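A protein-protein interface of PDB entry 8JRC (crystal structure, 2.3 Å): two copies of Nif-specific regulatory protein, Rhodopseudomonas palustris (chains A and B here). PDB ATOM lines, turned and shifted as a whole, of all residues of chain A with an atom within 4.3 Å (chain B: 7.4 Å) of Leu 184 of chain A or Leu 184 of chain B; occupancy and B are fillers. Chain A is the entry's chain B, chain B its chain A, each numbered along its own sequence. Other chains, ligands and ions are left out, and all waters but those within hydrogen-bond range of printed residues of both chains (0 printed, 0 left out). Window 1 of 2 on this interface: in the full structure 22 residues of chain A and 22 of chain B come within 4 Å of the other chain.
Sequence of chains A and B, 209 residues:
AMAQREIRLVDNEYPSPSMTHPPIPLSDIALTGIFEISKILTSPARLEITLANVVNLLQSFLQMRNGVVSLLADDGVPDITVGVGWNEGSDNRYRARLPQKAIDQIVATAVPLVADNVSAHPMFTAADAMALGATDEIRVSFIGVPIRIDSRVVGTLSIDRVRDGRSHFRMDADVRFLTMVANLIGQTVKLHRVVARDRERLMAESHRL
CG2 of Ile 34 of chain A touches SD of Met 180 of chain B, 3.8 Å away.
Ser 38 of chain A touches Met 180 of chain B (OG to CG, 3.7 Å).
Ser 38 of chain A touches Asn 183 of chain B (OG to ND2, 3.6 Å).
Leu 184 of chain B touches Ser 38 of chain A (CD2 to CB, 3.8 Å).
Met 180 of chain A touches Ser 38 of chain B.
Ser 38 of chain B touches Asn 183 of chain A.
O of Asn 183 of chain A touches CG2 of Thr 42 of chain B (3.2 Å).
Leu 184 of chain A touches Ser 38 of chain B.
Leu 184 of chain A touches Leu 184 of chain B (CD1 to CD1, 3.9 Å).
Gln 187 of chain B touches Leu 184 of chain A.
The backbone carbonyl oxygen (O) of Lys 39 of chain B lies within hydrogen-bond range of the side-chain hydroxyl (OG1) of Thr 42 of chain B, at 2.9 Å.
O of Phe 35 of chain B is in hydrogen-bond range of OG of Ser 38 of chain B (2.7 Å).
OG1 of Thr 188 of chain A is in hydrogen-bond range of O of Leu 184 of chain A, at 3.1 Å.
O of Leu 184 of chain B sits at hydrogen-bond distance from OG1 of Thr 188 of chain B.
The side-chain amide nitrogen (ND2) of Asn 183 of chain B lies close to the backbone carbonyl oxygen (O) of Thr 179 of chain B, 3.3 Å away.
Printed residues of chain B within 4 Å of Met 180 of chain A: Ile 34, Phe 35 and Ser 38.
Printed residues of chain B within 4 Å of Asn 183 of chain A: Ser 38 (3.6 Å) and Thr 42 (3.2 Å).
Of chain B, only Ser 38 (3.8 Å), Leu 184 (3.9 Å) and Gln 187 (3.9 Å) come within 4 Å of Leu 184 of chain A.
Of the printed residues of chain A, Leu 184 of chain B touches Ser 38, Leu 184 and Gln 187.
The nearest printed residue of chain A that does not touch Leu 184 of chain B is Leu 41 of chain A (5.1 Å).
Leu 41 of chain A touches Gln 187 of chain B, and with the chains exchanged Gln 187 of chain A touches Leu 41 of chain B.
Leu 184 of chain A touches its own counterpart, Leu 184 of chain B.
Leu 184 of chain A touches Gln 187 of chain B, and with the chains exchanged Gln 187 of chain A touches Leu 184 of chain B.
Gln 187 of chain B touches its own counterpart, Gln 187 of chain A.
Of the 18 pairs that touch across the chains among the printed residues, 16 have their exchanged pair printed and touching as well.
Printed residues of chain A that touch a printed residue of chain B: Ile 34, Ser 38, Leu 41, Met 180, Asn 183, Leu 184, Gln 187 and Thr 188.
Along chain A the printed residues that touch a printed residue of chain B span positions 34 to 188.
Hydrophobic or aromatic side chains of chain B that line the printed part of chain A: Ile 34, Leu 41, Met 180 and Leu 184.
Among the printed residues, 18 pairs touch across the chains.
The side-chain hydroxyl (OG1) of Thr 188 of chain A is in hydrogen-bond range of the side-chain amide oxygen (OE1) of Gln 187 of chain B, 2.9 Å away.
NE2 of Gln 187 of chain B lies within hydrogen-bond range of O of Leu 41 of chain A (3.1 Å).
The backbone NH (N) of Phe 35 of chain B lies close to the side-chain sulfur (SD) of Met 180 of chain A.
The backbone carbonyl oxygen (O) of Leu 41 of chain B sits close to the side-chain amide oxygen (OE1) of Gln 187 of chain A (3.4 Å).
OE1 of Gln 187 of chain A sits at hydrogen-bond distance from OG1 of Thr 188 of chain B, at 2.8 Å.
The side-chain amide nitrogen of Gln 187 of chain A sits at hydrogen-bond distance from the backbone carbonyl oxygen of Leu 184 of chain B (3.3 Å).
The backbone carbonyl oxygen (O) of Ile 34 of chain B lies close to the side-chain sulfur (SD) of Met 180 of chain A, at 3.8 Å.
The side-chain amide oxygen of Gln 187 of chain B lies within hydrogen-bond range of the side-chain amide nitrogen of Gln 187 of chain A (3.4 Å).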
ATOM      1  N   ILE A  34     -18.801  -8.640  13.544  1.00  0.00           N
ATOM      2  CA  ILE A  34     -18.040  -9.302  12.488  1.00  0.00           C
ATOM      3  C   ILE A  34     -16.757  -9.907  13.048  1.00  0.00           C
ATOM      4  O   ILE A  34     -16.298 -10.953  12.569  1.00  0.00           O
ATOM      5  CB  ILE A  34     -17.760  -8.327  11.326  1.00  0.00           C
ATOM      6  CG1 ILE A  34     -17.101  -9.062  10.156  1.00  0.00           C
ATOM      7  CG2 ILE A  34     -16.903  -7.157  11.778  1.00  0.00           C
ATOM      8  CD1 ILE A  34     -17.975 -10.137   9.543  1.00  0.00           C
ATOM      9  N   SER A  38     -16.082 -13.856  12.708  1.00  0.00           N
ATOM     10  CA  SER A  38     -14.866 -14.384  12.098  1.00  0.00           C
ATOM     11  C   SER A  38     -14.266 -15.512  12.930  1.00  0.00           C
ATOM     12  O   SER A  38     -13.735 -16.482  12.376  1.00  0.00           O
ATOM     13  CB  SER A  38     -13.848 -13.261  11.901  1.00  0.00           C
ATOM     14  OG  SER A  38     -12.990 -13.143  13.024  1.00  0.00           O
ATOM     15  N   LEU A  41     -16.518 -18.641  12.424  1.00  0.00           N
ATOM     16  CA  LEU A  41     -16.353 -19.279  11.121  1.00  0.00           C
ATOM     17  C   LEU A  41     -15.057 -20.072  11.029  1.00  0.00           C
ATOM     18  O   LEU A  41     -14.970 -21.021  10.241  1.00  0.00           O
ATOM     19  CB  LEU A  41     -16.402 -18.226  10.016  1.00  0.00           C
ATOM     20  CG  LEU A  41     -17.774 -17.612   9.740  1.00  0.00           C
ATOM     21  CD1 LEU A  41     -17.643 -16.434   8.793  1.00  0.00           C
ATOM     22  CD2 LEU A  41     -18.717 -18.655   9.170  1.00  0.00           C
ATOM     23  N   MET A 180     -21.372  -9.025   3.502  1.00  0.00           N
ATOM     24  CA  MET A 180     -20.056  -9.380   4.024  1.00  0.00           C
ATOM     25  C   MET A 180     -20.089 -10.739   4.715  1.00  0.00           C
ATOM     26  O   MET A 180     -19.231 -11.594   4.467  1.00  0.00           O
ATOM     27  CB  MET A 180     -19.573  -8.290   4.981  1.00  0.00           C
ATOM     28  CG  MET A 180     -18.354  -8.661   5.806  1.00  0.00           C
ATOM     29  SD  MET A 180     -17.726  -7.255   6.743  1.00  0.00           S
ATOM     30  CE  MET A 180     -19.138  -6.872   7.775  1.00  0.00           C
ATOM     31  N   VAL A 181     -21.078 -10.953   5.587  1.00  0.00           N
ATOM     32  CA  VAL A 181     -21.183 -12.223   6.303  1.00  0.00           C
ATOM     33  C   VAL A 181     -21.390 -13.373   5.326  1.00  0.00           C
ATOM     34  O   VAL A 181     -20.806 -14.453   5.482  1.00  0.00           O
ATOM     35  CB  VAL A 181     -22.314 -12.155   7.346  1.00  0.00           C
ATOM     36  CG1 VAL A 181     -22.534 -13.518   7.986  1.00  0.00           C
ATOM     37  CG2 VAL A 181     -21.993 -11.109   8.404  1.00  0.00           C
ATOM     38  N   ALA A 182     -22.216 -13.158   4.299  1.00  0.00           N
ATOM     39  CA  ALA A 182     -22.458 -14.206   3.312  1.00  0.00           C
ATOM     40  C   ALA A 182     -21.199 -14.521   2.514  1.00  0.00           C
ATOM     41  O   ALA A 182     -20.929 -15.690   2.212  1.00  0.00           O
ATOM     42  CB  ALA A 182     -23.594 -13.794   2.379  1.00  0.00           C
ATOM     43  N   ASN A 183     -20.427 -13.493   2.148  1.00  0.00           N
ATOM     44  CA  ASN A 183     -19.151 -13.721   1.477  1.00  0.00           C
ATOM     45  C   ASN A 183     -18.260 -14.650   2.290  1.00  0.00           C
ATOM     46  O   ASN A 183     -17.653 -15.581   1.747  1.00  0.00           O
ATOM     47  CB  ASN A 183     -18.438 -12.391   1.227  1.00  0.00           C
ATOM     48  CG  ASN A 183     -19.086 -11.578   0.126  1.00  0.00           C
ATOM     49  OD1 ASN A 183     -19.835 -12.107  -0.695  1.00  0.00           O
ATOM     50  ND2 ASN A 183     -18.800 -10.282   0.104  1.00  0.00           N
ATOM     51  N   LEU A 184     -18.180 -14.420   3.601  1.00  0.00           N
ATOM     52  CA  LEU A 184     -17.325 -15.243   4.447  1.00  0.00           C
ATOM     53  C   LEU A 184     -17.915 -16.634   4.645  1.00  0.00           C
ATOM     54  O   LEU A 184     -17.178 -17.625   4.695  1.00  0.00           O
ATOM     55  CB  LEU A 184     -17.098 -14.546   5.786  1.00  0.00           C
ATOM     56  CG  LEU A 184     -16.511 -13.139   5.668  1.00  0.00           C
ATOM     57  CD1 LEU A 184     -16.320 -12.508   7.036  1.00  0.00           C
ATOM     58  CD2 LEU A 184     -15.194 -13.172   4.900  1.00  0.00           C
ATOM     59  N   ILE A 185     -19.243 -16.728   4.769  1.00  0.00           N
ATOM     60  CA  ILE A 185     -19.892 -18.034   4.855  1.00  0.00           C
ATOM     61  C   ILE A 185     -19.568 -18.871   3.624  1.00  0.00           C
ATOM     62  O   ILE A 185     -19.278 -20.069   3.727  1.00  0.00           O
ATOM     63  CB  ILE A 185     -21.411 -17.869   5.044  1.00  0.00           C
ATOM     64  CG1 ILE A 185     -21.724 -17.341   6.445  1.00  0.00           C
ATOM     65  CG2 ILE A 185     -22.133 -19.188   4.796  1.00  0.00           C
ATOM     66  CD1 ILE A 185     -23.192 -17.033   6.659  1.00  0.00           C
ATOM     67  N   GLY A 186     -19.602 -18.249   2.442  1.00  0.00           N
ATOM     68  CA  GLY A 186     -19.270 -18.970   1.223  1.00  0.00           C
ATOM     69  C   GLY A 186     -17.880 -19.576   1.260  1.00  0.00           C
ATOM     70  O   GLY A 186     -17.681 -20.719   0.840  1.00  0.00           O
ATOM     71  N   GLN A 187     -16.899 -18.818   1.756  1.00  0.00           N
ATOM     72  CA  GLN A 187     -15.553 -19.360   1.915  1.00  0.00           C
ATOM     73  C   GLN A 187     -15.549 -20.542   2.878  1.00  0.00           C
ATOM     74  O   GLN A 187     -14.890 -21.557   2.626  1.00  0.00           O
ATOM     75  CB  GLN A 187     -14.602 -18.264   2.400  1.00  0.00           C
ATOM     76  CG  GLN A 187     -13.233 -18.763   2.837  1.00  0.00           C
ATOM     77  CD  GLN A 187     -12.198 -17.655   2.899  1.00  0.00           C
ATOM     78  OE1 GLN A 187     -11.671 -17.224   1.874  1.00  0.00           O
ATOM     79  NE2 GLN A 187     -11.901 -17.187   4.107  1.00  0.00           N
ATOM     80  N   THR A 188     -16.290 -20.430   3.983  1.00  0.00           N
ATOM     81  CA  THR A 188     -16.385 -21.533   4.933  1.00  0.00           C
ATOM     82  C   THR A 188     -17.062 -22.748   4.310  1.00  0.00           C
ATOM     83  O   THR A 188     -16.648 -23.890   4.547  1.00  0.00           O
ATOM     84  CB  THR A 188     -17.146 -21.083   6.180  1.00  0.00           C
ATOM     85  OG1 THR A 188     -16.549 -19.889   6.702  1.00  0.00           O
ATOM     86  CG2 THR A 188     -17.117 -22.169   7.246  1.00  0.00           C
ATOM     87  N   ILE B  34     -13.114  -3.992   6.285  1.00  0.00           N
ATOM     88  CA  ILE B  34     -13.369  -5.425   6.395  1.00  0.00           C
ATOM     89  C   ILE B  34     -14.445  -5.855   5.405  1.00  0.00           C
ATOM     90  O   ILE B  34     -14.445  -6.999   4.933  1.00  0.00           O
ATOM     91  CB  ILE B  34     -13.738  -5.801   7.844  1.00  0.00           C
ATOM     92  CG1 ILE B  34     -13.928  -7.314   7.983  1.00  0.00           C
ATOM     93  CG2 ILE B  34     -14.991  -5.065   8.298  1.00  0.00           C
ATOM     94  CD1 ILE B  34     -12.661  -8.111   7.775  1.00  0.00           C
ATOM     95  N   PHE B  35     -15.378  -4.959   5.075  1.00  0.00           N
ATOM     96  CA  PHE B  35     -16.325  -5.236   4.001  1.00  0.00           C
ATOM     97  C   PHE B  35     -15.591  -5.480   2.688  1.00  0.00           C
ATOM     98  O   PHE B  35     -15.860  -6.459   1.982  1.00  0.00           O
ATOM     99  CB  PHE B  35     -17.313  -4.075   3.865  1.00  0.00           C
ATOM    100  CG  PHE B  35     -18.200  -4.165   2.652  1.00  0.00           C
ATOM    101  CD1 PHE B  35     -19.343  -4.950   2.670  1.00  0.00           C
ATOM    102  CD2 PHE B  35     -17.899  -3.455   1.501  1.00  0.00           C
ATOM    103  CE1 PHE B  35     -20.164  -5.031   1.560  1.00  0.00           C
ATOM    104  CE2 PHE B  35     -18.715  -3.533   0.387  1.00  0.00           C
ATOM    105  CZ  PHE B  35     -19.851  -4.323   0.418  1.00  0.00           C
ATOM    106  N   ILE B  37     -12.379  -6.225   2.370  1.00  0.00           N
ATOM    107  CA  ILE B  37     -11.508  -7.386   2.532  1.00  0.00           C
ATOM    108  C   ILE B  37     -12.288  -8.673   2.295  1.00  0.00           C
ATOM    109  O   ILE B  37     -11.774  -9.626   1.693  1.00  0.00           O
ATOM    110  CB  ILE B  37     -10.847  -7.362   3.924  1.00  0.00           C
ATOM    111  CG1 ILE B  37      -9.672  -6.384   3.938  1.00  0.00           C
ATOM    112  CG2 ILE B  37     -10.375  -8.750   4.329  1.00  0.00           C
ATOM    113  CD1 ILE B  37      -9.116  -6.119   5.321  1.00  0.00           C
ATOM    114  N   SER B  38     -13.545  -8.716   2.747  1.00  0.00           N
ATOM    115  CA  SER B  38     -14.362  -9.909   2.553  1.00  0.00           C
ATOM    116  C   SER B  38     -14.591 -10.187   1.073  1.00  0.00           C
ATOM    117  O   SER B  38     -14.595 -11.347   0.646  1.00  0.00           O
ATOM    118  CB  SER B  38     -15.695  -9.759   3.288  1.00  0.00           C
ATOM    119  OG  SER B  38     -16.604  -8.954   2.557  1.00  0.00           O
ATOM    120  N   LYS B  39     -14.786  -9.136   0.275  1.00  0.00           N
ATOM    121  CA  LYS B  39     -14.899  -9.313  -1.170  1.00  0.00           C
ATOM    122  C   LYS B  39     -13.615  -9.889  -1.752  1.00  0.00           C
ATOM    123  O   LYS B  39     -13.649 -10.813  -2.574  1.00  0.00           O
ATOM    124  CB  LYS B  39     -15.241  -7.979  -1.837  1.00  0.00           C
ATOM    125  CG  LYS B  39     -16.503  -7.322  -1.308  1.00  0.00           C
ATOM    126  CD  LYS B  39     -16.508  -5.831  -1.594  1.00  0.00           C
ATOM    127  CE  LYS B  39     -16.990  -5.538  -3.005  1.00  0.00           C
ATOM    128  NZ  LYS B  39     -17.198  -4.080  -3.225  1.00  0.00           N
ATOM    129  N   LEU B  41     -11.309 -11.750  -0.431  1.00  0.00           N
ATOM    130  CA  LEU B  41     -11.050 -13.142  -0.083  1.00  0.00           C
ATOM    131  C   LEU B  41     -11.947 -14.114  -0.835  1.00  0.00           C
ATOM    132  O   LEU B  41     -11.611 -15.299  -0.931  1.00  0.00           O
ATOM    133  CB  LEU B  41     -11.218 -13.347   1.421  1.00  0.00           C
ATOM    134  CG  LEU B  41     -10.300 -12.515   2.314  1.00  0.00           C
ATOM    135  CD1 LEU B  41     -10.937 -12.313   3.676  1.00  0.00           C
ATOM    136  CD2 LEU B  41      -8.940 -13.177   2.444  1.00  0.00           C
ATOM    137  N   THR B  42     -13.076 -13.648  -1.365  1.00  0.00           N
ATOM    138  CA  THR B  42     -13.977 -14.508  -2.118  1.00  0.00           C
ATOM    139  C   THR B  42     -13.724 -14.462  -3.617  1.00  0.00           C
ATOM    140  O   THR B  42     -14.307 -15.266  -4.353  1.00  0.00           O
ATOM    141  CB  THR B  42     -15.434 -14.122  -1.842  1.00  0.00           C
ATOM    142  OG1 THR B  42     -15.693 -12.817  -2.372  1.00  0.00           O
ATOM    143  CG2 THR B  42     -15.698 -14.118  -0.351  1.00  0.00           C
ATOM    144  N   ILE B 147      -1.297 -16.264  12.531  1.00  0.00           N
ATOM    145  CA  ILE B 147      -2.234 -16.891  11.608  1.00  0.00           C
ATOM    146  C   ILE B 147      -2.334 -18.358  11.996  1.00  0.00           C
ATOM    147  O   ILE B 147      -1.317 -19.059  12.064  1.00  0.00           O
ATOM    148  CB  ILE B 147      -1.789 -16.731  10.146  1.00  0.00           C
ATOM    149  CG1 ILE B 147      -1.702 -15.249   9.771  1.00  0.00           C
ATOM    150  CG2 ILE B 147      -2.743 -17.465   9.215  1.00  0.00           C
ATOM    151  CD1 ILE B 147      -1.133 -14.998   8.392  1.00  0.00           C
ATOM    152  N   ARG B 148      -3.552 -18.823  12.262  1.00  0.00           N
ATOM    153  CA  ARG B 148      -3.779 -20.161  12.782  1.00  0.00           C
ATOM    154  C   ARG B 148      -4.682 -20.956  11.850  1.00  0.00           C
ATOM    155  O   ARG B 148      -5.591 -20.410  11.218  1.00  0.00           O
ATOM    156  CB  ARG B 148      -4.408 -20.116  14.181  1.00  0.00           C
ATOM    157  CG  ARG B 148      -3.410 -19.974  15.319  1.00  0.00           C
ATOM    158  CD  ARG B 148      -4.114 -19.570  16.604  1.00  0.00           C
ATOM    159  NE  ARG B 148      -4.863 -18.327  16.434  1.00  0.00           N
ATOM    160  CZ  ARG B 148      -5.794 -17.891  17.276  1.00  0.00           C
ATOM    161  NH1 ARG B 148      -6.101 -18.598  18.355  1.00  0.00           N
ATOM    162  NH2 ARG B 148      -6.421 -16.747  17.036  1.00  0.00           N
ATOM    163  N   LEU B 178      -6.590  -6.866  13.210  1.00  0.00           N
ATOM    164  CA  LEU B 178      -5.681  -7.785  12.531  1.00  0.00           C
ATOM    165  C   LEU B 178      -5.958  -9.230  12.924  1.00  0.00           C
ATOM    166  O   LEU B 178      -5.831 -10.138  12.094  1.00  0.00           O
ATOM    167  CB  LEU B 178      -4.230  -7.414  12.839  1.00  0.00           C
ATOM    168  CG  LEU B 178      -3.727  -6.070  12.310  1.00  0.00           C
ATOM    169  CD1 LEU B 178      -2.346  -5.767  12.872  1.00  0.00           C
ATOM    170  CD2 LEU B 178      -3.710  -6.048  10.789  1.00  0.00           C
ATOM    171  N   THR B 179      -6.321  -9.466  14.187  1.00  0.00           N
ATOM    172  CA  THR B 179      -6.705 -10.810  14.610  1.00  0.00           C
ATOM    173  C   THR B 179      -7.899 -11.312  13.809  1.00  0.00           C
ATOM    174  O   THR B 179      -7.963 -12.492  13.445  1.00  0.00           O
ATOM    175  CB  THR B 179      -7.014 -10.820  16.109  1.00  0.00           C
ATOM    176  OG1 THR B 179      -5.820 -10.516  16.846  1.00  0.00           O
ATOM    177  CG2 THR B 179      -7.547 -12.179  16.548  1.00  0.00           C
ATOM    178  N   MET B 180      -8.848 -10.423  13.507  1.00  0.00           N
ATOM    179  CA  MET B 180      -9.985 -10.801  12.676  1.00  0.00           C
ATOM    180  C   MET B 180      -9.539 -11.124  11.255  1.00  0.00           C
ATOM    181  O   MET B 180      -9.965 -12.128  10.671  1.00  0.00           O
ATOM    182  CB  MET B 180     -11.027  -9.681  12.676  1.00  0.00           C
ATOM    183  CG  MET B 180     -12.126  -9.849  11.641  1.00  0.00           C
ATOM    184  SD  MET B 180     -13.396  -8.577  11.782  1.00  0.00           S
ATOM    185  CE  MET B 180     -12.433  -7.102  11.462  1.00  0.00           C
ATOM    186  N   VAL B 181      -8.680 -10.278  10.682  1.00  0.00           N
ATOM    187  CA  VAL B 181      -8.181 -10.521   9.332  1.00  0.00           C
ATOM    188  C   VAL B 181      -7.363 -11.806   9.286  1.00  0.00           C
ATOM    189  O   VAL B 181      -7.464 -12.591   8.336  1.00  0.00           O
ATOM    190  CB  VAL B 181      -7.367  -9.310   8.839  1.00  0.00           C
ATOM    191  CG1 VAL B 181      -6.807  -9.571   7.453  1.00  0.00           C
ATOM    192  CG2 VAL B 181      -8.234  -8.056   8.841  1.00  0.00           C
ATOM    193  N   ALA B 182      -6.542 -12.042  10.314  1.00  0.00           N
ATOM    194  CA  ALA B 182      -5.717 -13.246  10.343  1.00  0.00           C
ATOM    195  C   ALA B 182      -6.573 -14.506  10.374  1.00  0.00           C
ATOM    196  O   ALA B 182      -6.264 -15.491   9.693  1.00  0.00           O
ATOM    197  CB  ALA B 182      -4.772 -13.206  11.543  1.00  0.00           C
ATOM    198  N   ASN B 183      -7.646 -14.499  11.171  1.00  0.00           N
ATOM    199  CA  ASN B 183      -8.564 -15.634  11.204  1.00  0.00           C
ATOM    200  C   ASN B 183      -9.089 -15.958   9.812  1.00  0.00           C
ATOM    201  O   ASN B 183      -9.051 -17.112   9.371  1.00  0.00           O
ATOM    202  CB  ASN B 183      -9.728 -15.344  12.153  1.00  0.00           C
ATOM    203  CG  ASN B 183      -9.309 -15.320  13.605  1.00  0.00           C
ATOM    204  OD1 ASN B 183      -8.257 -15.846  13.970  1.00  0.00           O
ATOM    205  ND2 ASN B 183     -10.135 -14.709  14.445  1.00  0.00           N
ATOM    206  N   LEU B 184      -9.584 -14.940   9.105  1.00  0.00           N
ATOM    207  CA  LEU B 184     -10.128 -15.159   7.770  1.00  0.00           C
ATOM    208  C   LEU B 184      -9.045 -15.606   6.795  1.00  0.00           C
ATOM    209  O   LEU B 184      -9.286 -16.474   5.949  1.00  0.00           O
ATOM    210  CB  LEU B 184     -10.816 -13.887   7.274  1.00  0.00           C
ATOM    211  CG  LEU B 184     -11.926 -13.346   8.181  1.00  0.00           C
ATOM    212  CD1 LEU B 184     -12.483 -12.037   7.648  1.00  0.00           C
ATOM    213  CD2 LEU B 184     -13.033 -14.376   8.344  1.00  0.00           C
ATOM    214  N   ILE B 185      -7.847 -15.023   6.897  1.00  0.00           N
ATOM    215  CA  ILE B 185      -6.750 -15.419   6.018  1.00  0.00           C
ATOM    216  C   ILE B 185      -6.393 -16.884   6.237  1.00  0.00           C
ATOM    217  O   ILE B 185      -6.118 -17.621   5.282  1.00  0.00           O
ATOM    218  CB  ILE B 185      -5.535 -14.496   6.232  1.00  0.00           C
ATOM    219  CG1 ILE B 185      -5.799 -13.122   5.615  1.00  0.00           C
ATOM    220  CG2 ILE B 185      -4.273 -15.109   5.642  1.00  0.00           C
ATOM    221  CD1 ILE B 185      -4.706 -12.119   5.887  1.00  0.00           C
ATOM    222  N   GLY B 186      -6.400 -17.331   7.495  1.00  0.00           N
ATOM    223  CA  GLY B 186      -6.156 -18.738   7.772  1.00  0.00           C
ATOM    224  C   GLY B 186      -7.134 -19.652   7.062  1.00  0.00           C
ATOM    225  O   GLY B 186      -6.755 -20.713   6.559  1.00  0.00           O
ATOM    226  N   GLN B 187      -8.409 -19.257   7.014  1.00  0.00           N
ATOM    227  CA  GLN B 187      -9.396 -20.033   6.270  1.00  0.00           C
ATOM    228  C   GLN B 187      -9.091 -20.021   4.778  1.00  0.00           C
ATOM    229  O   GLN B 187      -9.207 -21.051   4.103  1.00  0.00           O
ATOM    230  CB  GLN B 187     -10.800 -19.490   6.540  1.00  0.00           C
ATOM    231  CG  GLN B 187     -11.925 -20.325   5.945  1.00  0.00           C
ATOM    232  CD  GLN B 187     -13.278 -19.985   6.540  1.00  0.00           C
ATOM    233  OE1 GLN B 187     -13.838 -18.921   6.272  1.00  0.00           O
ATOM    234  NE2 GLN B 187     -13.811 -20.887   7.356  1.00  0.00           N
ATOM    235  N   THR B 188      -8.699 -18.860   4.245  1.00  0.00           N
ATOM    236  CA  THR B 188      -8.316 -18.779   2.839  1.00  0.00           C
ATOM    237  C   THR B 188      -7.100 -19.648   2.551  1.00  0.00           C
ATOM    238  O   THR B 188      -7.018 -20.287   1.495  1.00  0.00           O
ATOM    239  CB  THR B 188      -8.037 -17.327   2.450  1.00  0.00           C
ATOM    240  OG1 THR B 188      -9.153 -16.507   2.817  1.00  0.00           O
ATOM    241  CG2 THR B 188      -7.797 -17.211   0.951  1.00  0.00           C
ATOM    242  N   VAL B 189      -6.145 -19.688   3.482  1.00  0.00           N
ATOM    243  CA  VAL B 189      -4.940 -20.485   3.281  1.00  0.00           C
ATOM    244  C   VAL B 189      -5.266 -21.971   3.363  1.00  0.00           C
ATOM    245  O   VAL B 189      -4.831 -22.764   2.519  1.00  0.00           O
ATOM    246  CB  VAL B 189      -3.856 -20.085   4.297  1.00  0.00           C
ATOM    247  CG1 VAL B 189      -2.685 -21.051   4.235  1.00  0.00           C
ATOM    248  CG2 VAL B 189      -3.390 -18.663   4.036  1.00  0.00           C
ATOM    249  N   LYS B 190      -6.031 -22.372   4.382  1.00  0.00           N
ATOM    250  CA  LYS B 190      -6.437 -23.771   4.485  1.00  0.00           C
ATOM    251  C   LYS B 190      -7.193 -24.211   3.240  1.00  0.00           C
ATOM    252  O   LYS B 190      -6.985 -25.322   2.740  1.00  0.00           O
ATOM    253  CB  LYS B 190      -7.290 -23.992   5.735  1.00  0.00           C
ATOM    254  CG  LYS B 190      -7.519 -25.463   6.055  1.00  0.00           C
ATOM    255  CD  LYS B 190      -8.587 -25.661   7.121  1.00  0.00           C
ATOM    256  CE  LYS B 190      -8.898 -27.139   7.308  1.00  0.00           C
ATOM    257  NZ  LYS B 190      -9.929 -27.375   8.357  1.00  0.00           N
